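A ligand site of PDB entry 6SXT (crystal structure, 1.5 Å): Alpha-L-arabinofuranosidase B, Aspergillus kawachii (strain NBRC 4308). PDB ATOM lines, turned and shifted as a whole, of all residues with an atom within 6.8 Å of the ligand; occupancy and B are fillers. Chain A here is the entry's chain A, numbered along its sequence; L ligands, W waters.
Water W1 lies within hydrogen-bond range of N1 of the ligand (2.6 Å), OG of Ser 283 (2.8 Å) and SG of Cys 160 (3.5 Å).
Merely in contact with the ligand: Cys 161 (3.8 Å), Asp 163 (3.9 Å), Asp 173 (3.8 Å), Trp 190 (3.9 Å) and Gly 279 (3.2 Å).
Hydrophobic or aromatic side chains that line the ligand: Met 179 and Trp 190.
13 residues have an atom within 4 Å of the ligand: Cys 160, Cys 161, Asp 163, Asp 173, Met 179, Trp 190, Asp 203, Glu 205, Asn 206, Asn 207, Gly 279, Gly 280 and Asp 281.
An oxygen (O1) of the ligand sits at hydrogen-bond distance from the backbone NH (N) of Asp 281.
An oxygen (O1) of the ligand sits at hydrogen-bond distance from the side-chain sulfur (SD) of Met 179 (3.1 Å).
OD2 of Asp 281 is in salt-bridge range of N1 of the ligand (3.2 Å).
The backbone NH (N) of Asn 206 sits at hydrogen-bond distance from an oxygen (O3) of the ligand (2.9 Å).
The side-chain sulfur (SG) of Cys 160 sits at hydrogen-bond distance from an oxygen (O2) of the ligand (3.8 Å).
The side-chain carboxylate (OE2) of Glu 205 is covalently linked to a carbon (C1) of the ligand (1.4 Å).
An oxygen (O1) of the ligand sits at hydrogen-bond distance from the backbone NH of Gly 280, 2.9 Å away.
N of Asn 207 sits at hydrogen-bond distance from O3 of the ligand (3.1 Å).
OD2 of Asp 203 lies within hydrogen-bond range of O2 of the ligand, at 2.6 Å.
The backbone carbonyl oxygen of Asp 281 is in hydrogen-bond range of the backbone NH of Phe 93, 3.0 Å away.
OH of Tyr 265 lies within hydrogen-bond range of O of Glu 205 (2.7 Å).
N of Gly 279 sits at hydrogen-bond distance from O of Cys 161 (3.5 Å).
SG of Cys 160 is disulfide-bonded to SG of Cys 161.
The backbone NH (N) of Gly 280 lies close to the side-chain sulfur (SD) of Met 179, 3.6 Å away.
The side-chain sulfur (SG) of Cys 160 sits close to the side-chain hydroxyl (OG) of Ser 283, at 3.7 Å.
OD1 of Asp 281 is in hydrogen-bond range of OG of Ser 283.
The side-chain carboxylate of Glu 205 sits close to the side-chain carboxylate of Glu 168, 2.7 Å away.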
ATOM      1  N   PHE A  93      11.679  22.674 -26.977  1.00  0.00           N
ATOM      2  CA  PHE A  93      10.732  23.293 -26.048  1.00  0.00           C
ATOM      3  C   PHE A  93       9.809  24.205 -26.821  1.00  0.00           C
ATOM      4  O   PHE A  93      10.192  24.841 -27.845  1.00  0.00           O
ATOM      5  CB  PHE A  93      11.486  24.074 -24.963  1.00  0.00           C
ATOM      6  CG  PHE A  93      12.328  23.214 -24.069  1.00  0.00           C
ATOM      7  CD1 PHE A  93      11.769  22.644 -22.940  1.00  0.00           C
ATOM      8  CD2 PHE A  93      13.645  22.976 -24.363  1.00  0.00           C
ATOM      9  CE1 PHE A  93      12.555  21.876 -22.089  1.00  0.00           C
ATOM     10  CE2 PHE A  93      14.430  22.171 -23.546  1.00  0.00           C
ATOM     11  CZ  PHE A  93      13.873  21.621 -22.407  1.00  0.00           C
ATOM     12  N   CYS A 160      17.942  28.417 -18.561  1.00  0.00           N
ATOM     13  CA  CYS A 160      18.523  28.220 -19.892  1.00  0.00           C
ATOM     14  C   CYS A 160      17.624  28.910 -20.924  1.00  0.00           C
ATOM     15  O   CYS A 160      16.409  28.674 -20.903  1.00  0.00           O
ATOM     16  CB  CYS A 160      18.633  26.757 -20.235  1.00  0.00           C
ATOM     17  SG  CYS A 160      19.466  26.492 -21.800  1.00  0.00           S
ATOM     18  N   CYS A 161      18.160  29.749 -21.808  1.00  0.00           N
ATOM     19  CA  CYS A 161      19.532  30.180 -21.892  1.00  0.00           C
ATOM     20  C   CYS A 161      19.553  31.513 -22.645  1.00  0.00           C
ATOM     21  O   CYS A 161      18.867  31.607 -23.676  1.00  0.00           O
ATOM     22  CB  CYS A 161      20.469  29.281 -22.696  1.00  0.00           C
ATOM     23  SG  CYS A 161      21.110  27.825 -21.788  1.00  0.00           S
ATOM     24  N   ASP A 163      21.252  33.402 -24.997  1.00  0.00           N
ATOM     25  CA  ASP A 163      22.312  33.156 -25.974  1.00  0.00           C
ATOM     26  C   ASP A 163      22.238  34.133 -27.156  1.00  0.00           C
ATOM     27  O   ASP A 163      21.170  34.595 -27.535  1.00  0.00           O
ATOM     28  CB  ASP A 163      22.355  31.763 -26.559  1.00  0.00           C
ATOM     29  CG  ASP A 163      22.733  30.649 -25.623  1.00  0.00           C
ATOM     30  OD1 ASP A 163      23.009  30.900 -24.436  1.00  0.00           O
ATOM     31  OD2 ASP A 163      22.679  29.446 -26.119  1.00  0.00           O
ATOM     32  N   ALA A 167      23.663  28.157 -33.931  1.00  0.00           N
ATOM     33  CA  ALA A 167      22.835  27.096 -33.369  1.00  0.00           C
ATOM     34  C   ALA A 167      22.297  26.135 -34.436  1.00  0.00           C
ATOM     35  O   ALA A 167      22.676  26.240 -35.573  1.00  0.00           O
ATOM     36  CB  ALA A 167      21.756  27.672 -32.519  1.00  0.00           C
ATOM     37  N   GLU A 168      21.397  25.269 -33.984  1.00  0.00           N
ATOM     38  CA  GLU A 168      20.870  24.174 -34.803  1.00  0.00           C
ATOM     39  C   GLU A 168      19.759  24.673 -35.713  1.00  0.00           C
ATOM     40  O   GLU A 168      18.892  25.450 -35.271  1.00  0.00           O
ATOM     41  CB  GLU A 168      20.298  23.110 -33.898  1.00  0.00           C
ATOM     42  CG  GLU A 168      21.347  22.419 -33.065  1.00  0.00           C
ATOM     43  CD  GLU A 168      21.437  22.931 -31.637  1.00  0.00           C
ATOM     44  OE1 GLU A 168      21.056  24.101 -31.423  1.00  0.00           O
ATOM     45  OE2 GLU A 168      21.851  22.118 -30.762  1.00  0.00           O
ATOM     46  N   THR A 172      16.250  22.039 -32.372  1.00  0.00           N
ATOM     47  CA  THR A 172      16.325  20.924 -31.411  1.00  0.00           C
ATOM     48  C   THR A 172      17.775  20.616 -31.054  1.00  0.00           C
ATOM     49  O   THR A 172      18.704  21.071 -31.743  1.00  0.00           O
ATOM     50  CB  THR A 172      15.664  19.630 -31.979  1.00  0.00           C
ATOM     51  OG1 THR A 172      16.496  19.102 -33.015  1.00  0.00           O
ATOM     52  CG2 THR A 172      14.269  19.909 -32.493  1.00  0.00           C
ATOM     53  N   ASP A 173      17.946  19.888 -29.941  1.00  0.00           N
ATOM     54  CA  ASP A 173      19.278  19.467 -29.462  1.00  0.00           C
ATOM     55  C   ASP A 173      19.771  18.315 -30.337  1.00  0.00           C
ATOM     56  O   ASP A 173      19.282  17.192 -30.143  1.00  0.00           O
ATOM     57  CB  ASP A 173      19.189  19.095 -27.995  1.00  0.00           C
ATOM     58  CG  ASP A 173      20.505  18.717 -27.354  1.00  0.00           C
ATOM     59  OD1 ASP A 173      21.482  18.432 -28.094  1.00  0.00           O
ATOM     60  OD2 ASP A 173      20.501  18.607 -26.106  1.00  0.00           O
ATOM     61  N   THR A 174      20.699  18.582 -31.218  1.00  0.00           N
ATOM     62  CA  THR A 174      21.352  17.589 -32.096  1.00  0.00           C
ATOM     63  C   THR A 174      22.723  17.184 -31.568  1.00  0.00           C
ATOM     64  O   THR A 174      23.444  16.506 -32.314  1.00  0.00           O
ATOM     65  CB  THR A 174      21.368  18.116 -33.527  1.00  0.00           C
ATOM     66  OG1 THR A 174      22.076  19.371 -33.506  1.00  0.00           O
ATOM     67  CG2 THR A 174      19.964  18.298 -34.048  1.00  0.00           C
ATOM     68  N   MET A 179      26.402  23.787 -31.421  1.00  0.00           N
ATOM     69  CA  MET A 179      26.151  25.207 -31.077  1.00  0.00           C
ATOM     70  C   MET A 179      27.493  25.868 -30.807  1.00  0.00           C
ATOM     71  O   MET A 179      28.460  25.226 -30.357  1.00  0.00           O
ATOM     72  CB  MET A 179      25.316  25.337 -29.798  1.00  0.00           C
ATOM     73  CG  MET A 179      23.847  25.207 -30.076  1.00  0.00           C
ATOM     74  SD  MET A 179      22.875  25.271 -28.577  1.00  0.00           S
ATOM     75  CE  MET A 179      23.086  27.021 -28.258  1.00  0.00           C
ATOM     76  N   TRP A 190      25.721  23.823 -15.731  1.00  0.00           N
ATOM     77  CA  TRP A 190      26.916  23.329 -16.427  1.00  0.00           C
ATOM     78  C   TRP A 190      28.133  24.092 -15.905  1.00  0.00           C
ATOM     79  O   TRP A 190      28.684  23.766 -14.850  1.00  0.00           O
ATOM     80  CB  TRP A 190      26.668  23.472 -17.950  1.00  0.00           C
ATOM     81  CG  TRP A 190      25.447  22.766 -18.465  1.00  0.00           C
ATOM     82  CD1 TRP A 190      25.359  21.442 -18.838  1.00  0.00           C
ATOM     83  CD2 TRP A 190      24.161  23.339 -18.737  1.00  0.00           C
ATOM     84  NE1 TRP A 190      24.090  21.177 -19.280  1.00  0.00           N
ATOM     85  CE2 TRP A 190      23.321  22.308 -19.207  1.00  0.00           C
ATOM     86  CE3 TRP A 190      23.597  24.631 -18.560  1.00  0.00           C
ATOM     87  CZ2 TRP A 190      21.993  22.544 -19.561  1.00  0.00           C
ATOM     88  CZ3 TRP A 190      22.290  24.860 -18.935  1.00  0.00           C
ATOM     89  CH2 TRP A 190      21.494  23.821 -19.416  1.00  0.00           C
ATOM     90  N   VAL A 202      30.281  30.158 -23.079  1.00  0.00           N
ATOM     91  CA  VAL A 202      30.013  29.752 -24.475  1.00  0.00           C
ATOM     92  C   VAL A 202      29.136  28.512 -24.426  1.00  0.00           C
ATOM     93  O   VAL A 202      29.541  27.508 -23.823  1.00  0.00           O
ATOM     94  CB  VAL A 202      31.272  29.535 -25.297  1.00  0.00           C
ATOM     95  CG1 VAL A 202      30.971  29.033 -26.695  1.00  0.00           C
ATOM     96  CG2 VAL A 202      32.083  30.832 -25.345  1.00  0.00           C
ATOM     97  N   ASP A 203      28.013  28.615 -25.086  1.00  0.00           N
ATOM     98  CA  ASP A 203      27.068  27.478 -25.217  1.00  0.00           C
ATOM     99  C   ASP A 203      27.539  26.684 -26.409  1.00  0.00           C
ATOM    100  O   ASP A 203      27.475  27.150 -27.562  1.00  0.00           O
ATOM    101  CB  ASP A 203      25.638  27.982 -25.349  1.00  0.00           C
ATOM    102  CG  ASP A 203      24.572  26.922 -25.216  1.00  0.00           C
ATOM    103  OD1 ASP A 203      25.002  25.707 -25.216  1.00  0.00           O
ATOM    104  OD2 ASP A 203      23.376  27.332 -25.013  1.00  0.00           O
ATOM    105  N   MET A 204      27.975  25.436 -26.140  1.00  0.00           N
ATOM    106  CA  MET A 204      28.431  24.510 -27.201  1.00  0.00           C
ATOM    107  C   MET A 204      27.459  23.323 -27.299  1.00  0.00           C
ATOM    108  O   MET A 204      27.798  22.392 -28.036  1.00  0.00           O
ATOM    109  CB  MET A 204      29.852  24.030 -26.937  1.00  0.00           C
ATOM    110  CG  MET A 204      30.861  25.156 -26.974  1.00  0.00           C
ATOM    111  SD  MET A 204      32.574  24.525 -27.023  1.00  0.00           S
ATOM    112  CE  MET A 204      33.458  26.004 -26.519  1.00  0.00           C
ATOM    113  N   GLU A 205      26.316  23.428 -26.660  1.00  0.00           N
ATOM    114  CA  GLU A 205      25.225  22.429 -26.542  1.00  0.00           C
ATOM    115  C   GLU A 205      25.633  21.349 -25.512  1.00  0.00           C
ATOM    116  O   GLU A 205      26.754  20.802 -25.584  1.00  0.00           O
ATOM    117  CB  GLU A 205      24.874  21.830 -27.903  1.00  0.00           C
ATOM    118  CG  GLU A 205      23.648  20.917 -27.881  1.00  0.00           C
ATOM    119  CD  GLU A 205      22.343  21.535 -27.415  1.00  0.00           C
ATOM    120  OE1 GLU A 205      21.403  21.726 -28.179  1.00  0.00           O
ATOM    121  OE2 GLU A 205      22.207  21.953 -26.091  1.00  0.00           O
ATOM    122  N   ASN A 206      24.694  21.108 -24.621  1.00  0.00           N
ATOM    123  CA  ASN A 206      24.814  20.222 -23.436  1.00  0.00           C
ATOM    124  C   ASN A 206      25.983  20.694 -22.587  1.00  0.00           C
ATOM    125  O   ASN A 206      26.559  19.912 -21.818  1.00  0.00           O
ATOM    126  CB  ASN A 206      24.971  18.751 -23.861  1.00  0.00           C
ATOM    127  CG  ASN A 206      23.874  18.307 -24.806  1.00  0.00           C
ATOM    128  OD1 ASN A 206      24.158  17.554 -25.732  1.00  0.00           O
ATOM    129  ND2 ASN A 206      22.646  18.732 -24.598  1.00  0.00           N
ATOM    130  N   ASN A 207      26.250  21.984 -22.608  1.00  0.00           N
ATOM    131  CA  ASN A 207      27.310  22.597 -21.787  1.00  0.00           C
ATOM    132  C   ASN A 207      27.318  24.107 -22.092  1.00  0.00           C
ATOM    133  O   ASN A 207      27.438  24.436 -23.245  1.00  0.00           O
ATOM    134  CB  ASN A 207      28.693  22.007 -22.017  1.00  0.00           C
ATOM    135  CG  ASN A 207      29.136  21.016 -20.948  1.00  0.00           C
ATOM    136  OD1 ASN A 207      28.989  21.246 -19.738  1.00  0.00           O
ATOM    137  ND2 ASN A 207      29.566  19.847 -21.408  1.00  0.00           N
ATOM    138  N   LEU A 208      27.327  24.888 -21.015  1.00  0.00           N
ATOM    139  CA  LEU A 208      27.834  26.275 -21.039  1.00  0.00           C
ATOM    140  C   LEU A 208      29.229  26.187 -20.455  1.00  0.00           C
ATOM    141  O   LEU A 208      29.378  25.619 -19.343  1.00  0.00           O
ATOM    142  CB  LEU A 208      26.931  27.149 -20.192  1.00  0.00           C
ATOM    143  CG  LEU A 208      25.449  27.175 -20.535  1.00  0.00           C
ATOM    144  CD1 LEU A 208      24.703  28.085 -19.579  1.00  0.00           C
ATOM    145  CD2 LEU A 208      25.203  27.592 -21.953  1.00  0.00           C
ATOM    146  N   TYR A 265      33.118  17.859 -28.633  1.00  0.00           N
ATOM    147  CA  TYR A 265      33.467  19.299 -28.811  1.00  0.00           C
ATOM    148  C   TYR A 265      34.649  19.534 -29.712  1.00  0.00           C
ATOM    149  O   TYR A 265      35.046  20.690 -29.955  1.00  0.00           O
ATOM    150  CB  TYR A 265      33.633  19.941 -27.435  1.00  0.00           C
ATOM    151  CG  TYR A 265      32.382  19.862 -26.627  1.00  0.00           C
ATOM    152  CD1 TYR A 265      31.248  20.588 -26.968  1.00  0.00           C
ATOM    153  CD2 TYR A 265      32.246  19.010 -25.543  1.00  0.00           C
ATOM    154  CE1 TYR A 265      30.079  20.508 -26.251  1.00  0.00           C
ATOM    155  CE2 TYR A 265      31.082  18.893 -24.824  1.00  0.00           C
ATOM    156  CZ  TYR A 265      29.978  19.649 -25.158  1.00  0.00           C
ATOM    157  OH  TYR A 265      28.866  19.526 -24.426  1.00  0.00           O
ATOM    158  N   ILE A 275      20.568  32.350 -33.178  1.00  0.00           N
ATOM    159  CA  ILE A 275      19.574  32.497 -32.100  1.00  0.00           C
ATOM    160  C   ILE A 275      19.857  33.766 -31.311  1.00  0.00           C
ATOM    161  O   ILE A 275      21.048  34.193 -31.257  1.00  0.00           O
ATOM    162  CB  ILE A 275      19.550  31.297 -31.141  1.00  0.00           C
ATOM    163  CG1 ILE A 275      20.932  30.994 -30.590  1.00  0.00           C
ATOM    164  CG2 ILE A 275      18.871  30.101 -31.819  1.00  0.00           C
ATOM    165  CD1 ILE A 275      21.016  29.837 -29.606  1.00  0.00           C
ATOM    166  N   ILE A 278      17.596  32.743 -26.416  1.00  0.00           N
ATOM    167  CA  ILE A 278      17.087  31.365 -26.203  1.00  0.00           C
ATOM    168  C   ILE A 278      18.213  30.380 -26.425  1.00  0.00           C
ATOM    169  O   ILE A 278      19.258  30.724 -27.016  1.00  0.00           O
ATOM    170  CB  ILE A 278      15.936  31.092 -27.187  1.00  0.00           C
ATOM    171  CG1 ILE A 278      16.355  31.396 -28.628  1.00  0.00           C
ATOM    172  CG2 ILE A 278      14.695  31.834 -26.768  1.00  0.00           C
ATOM    173  CD1 ILE A 278      15.476  30.781 -29.660  1.00  0.00           C
ATOM    174  N   GLY A 279      18.029  29.142 -25.963  1.00  0.00           N
ATOM    175  CA  GLY A 279      18.952  28.074 -26.341  1.00  0.00           C
ATOM    176  C   GLY A 279      18.641  27.463 -27.685  1.00  0.00           C
ATOM    177  O   GLY A 279      17.603  27.826 -28.327  1.00  0.00           O
ATOM    178  N   GLY A 280      19.555  26.650 -28.184  1.00  0.00           N
ATOM    179  CA  GLY A 280      19.412  26.118 -29.542  1.00  0.00           C
ATOM    180  C   GLY A 280      18.227  25.166 -29.657  1.00  0.00           C
ATOM    181  O   GLY A 280      17.662  25.088 -30.757  1.00  0.00           O
ATOM    182  N   ASP A 281      17.805  24.567 -28.554  1.00  0.00           N
ATOM    183  CA  ASP A 281      16.597  23.690 -28.524  1.00  0.00           C
ATOM    184  C   ASP A 281      15.343  24.479 -28.194  1.00  0.00           C
ATOM    185  O   ASP A 281      14.260  23.932 -27.858  1.00  0.00           O
ATOM    186  CB  ASP A 281      16.814  22.544 -27.538  1.00  0.00           C
ATOM    187  CG  ASP A 281      17.121  22.996 -26.132  1.00  0.00           C
ATOM    188  OD1 ASP A 281      17.086  24.244 -25.861  1.00  0.00           O
ATOM    189  OD2 ASP A 281      17.450  22.123 -25.310  1.00  0.00           O
ATOM    190  N   ASN A 282      15.405  25.814 -28.267  1.00  0.00           N
ATOM    191  CA  ASN A 282      14.331  26.741 -27.883  1.00  0.00           C
ATOM    192  C   ASN A 282      14.119  26.772 -26.363  1.00  0.00           C
ATOM    193  O   ASN A 282      13.062  27.219 -25.953  1.00  0.00           O
ATOM    194  CB  ASN A 282      13.005  26.560 -28.663  1.00  0.00           C
ATOM    195  CG  ASN A 282      12.110  27.761 -28.508  1.00  0.00           C
ATOM    196  OD1 ASN A 282      10.877  27.669 -28.195  1.00  0.00           O
ATOM    197  ND2 ASN A 282      12.744  28.921 -28.681  1.00  0.00           N
ATOM    198  N   SER A 283      15.081  26.379 -25.554  1.00  0.00           N
ATOM    199  CA  SER A 283      15.014  26.659 -24.112  1.00  0.00           C
ATOM    200  C   SER A 283      14.716  28.144 -23.973  1.00  0.00           C
ATOM    201  O   SER A 283      15.508  28.934 -24.513  1.00  0.00           O
ATOM    202  CB  SER A 283      16.277  26.291 -23.382  1.00  0.00           C
ATOM    203  OG  SER A 283      16.500  24.870 -23.370  1.00  0.00           O
HETATM  204  C1  LIG L   1      20.969  22.347 -25.586  1.00  0.00           C
HETATM  205  C2  LIG L   1      20.487  23.769 -25.870  1.00  0.00           C
HETATM  206  O1  LIG L   1      20.396  24.027 -27.223  1.00  0.00           O
HETATM  207  C3  LIG L   1      21.523  24.558 -25.191  1.00  0.00           C
HETATM  208  O2  LIG L   1      21.110  25.984 -25.152  1.00  0.00           O
HETATM  209  C4  LIG L   1      21.490  23.948 -23.810  1.00  0.00           C
HETATM  210  C5  LIG L   1      22.785  24.145 -23.037  1.00  0.00           C
HETATM  211  O3  LIG L   1      23.939  23.715 -23.722  1.00  0.00           O
HETATM  212  C6  LIG L   1      21.171  22.426 -24.094  1.00  0.00           C
HETATM  213  N1  LIG L   1      19.929  22.125 -23.338  1.00  0.00           N
HETATM  214  O   HOH W   1      18.145  23.298 -21.773  1.00  0.00           O
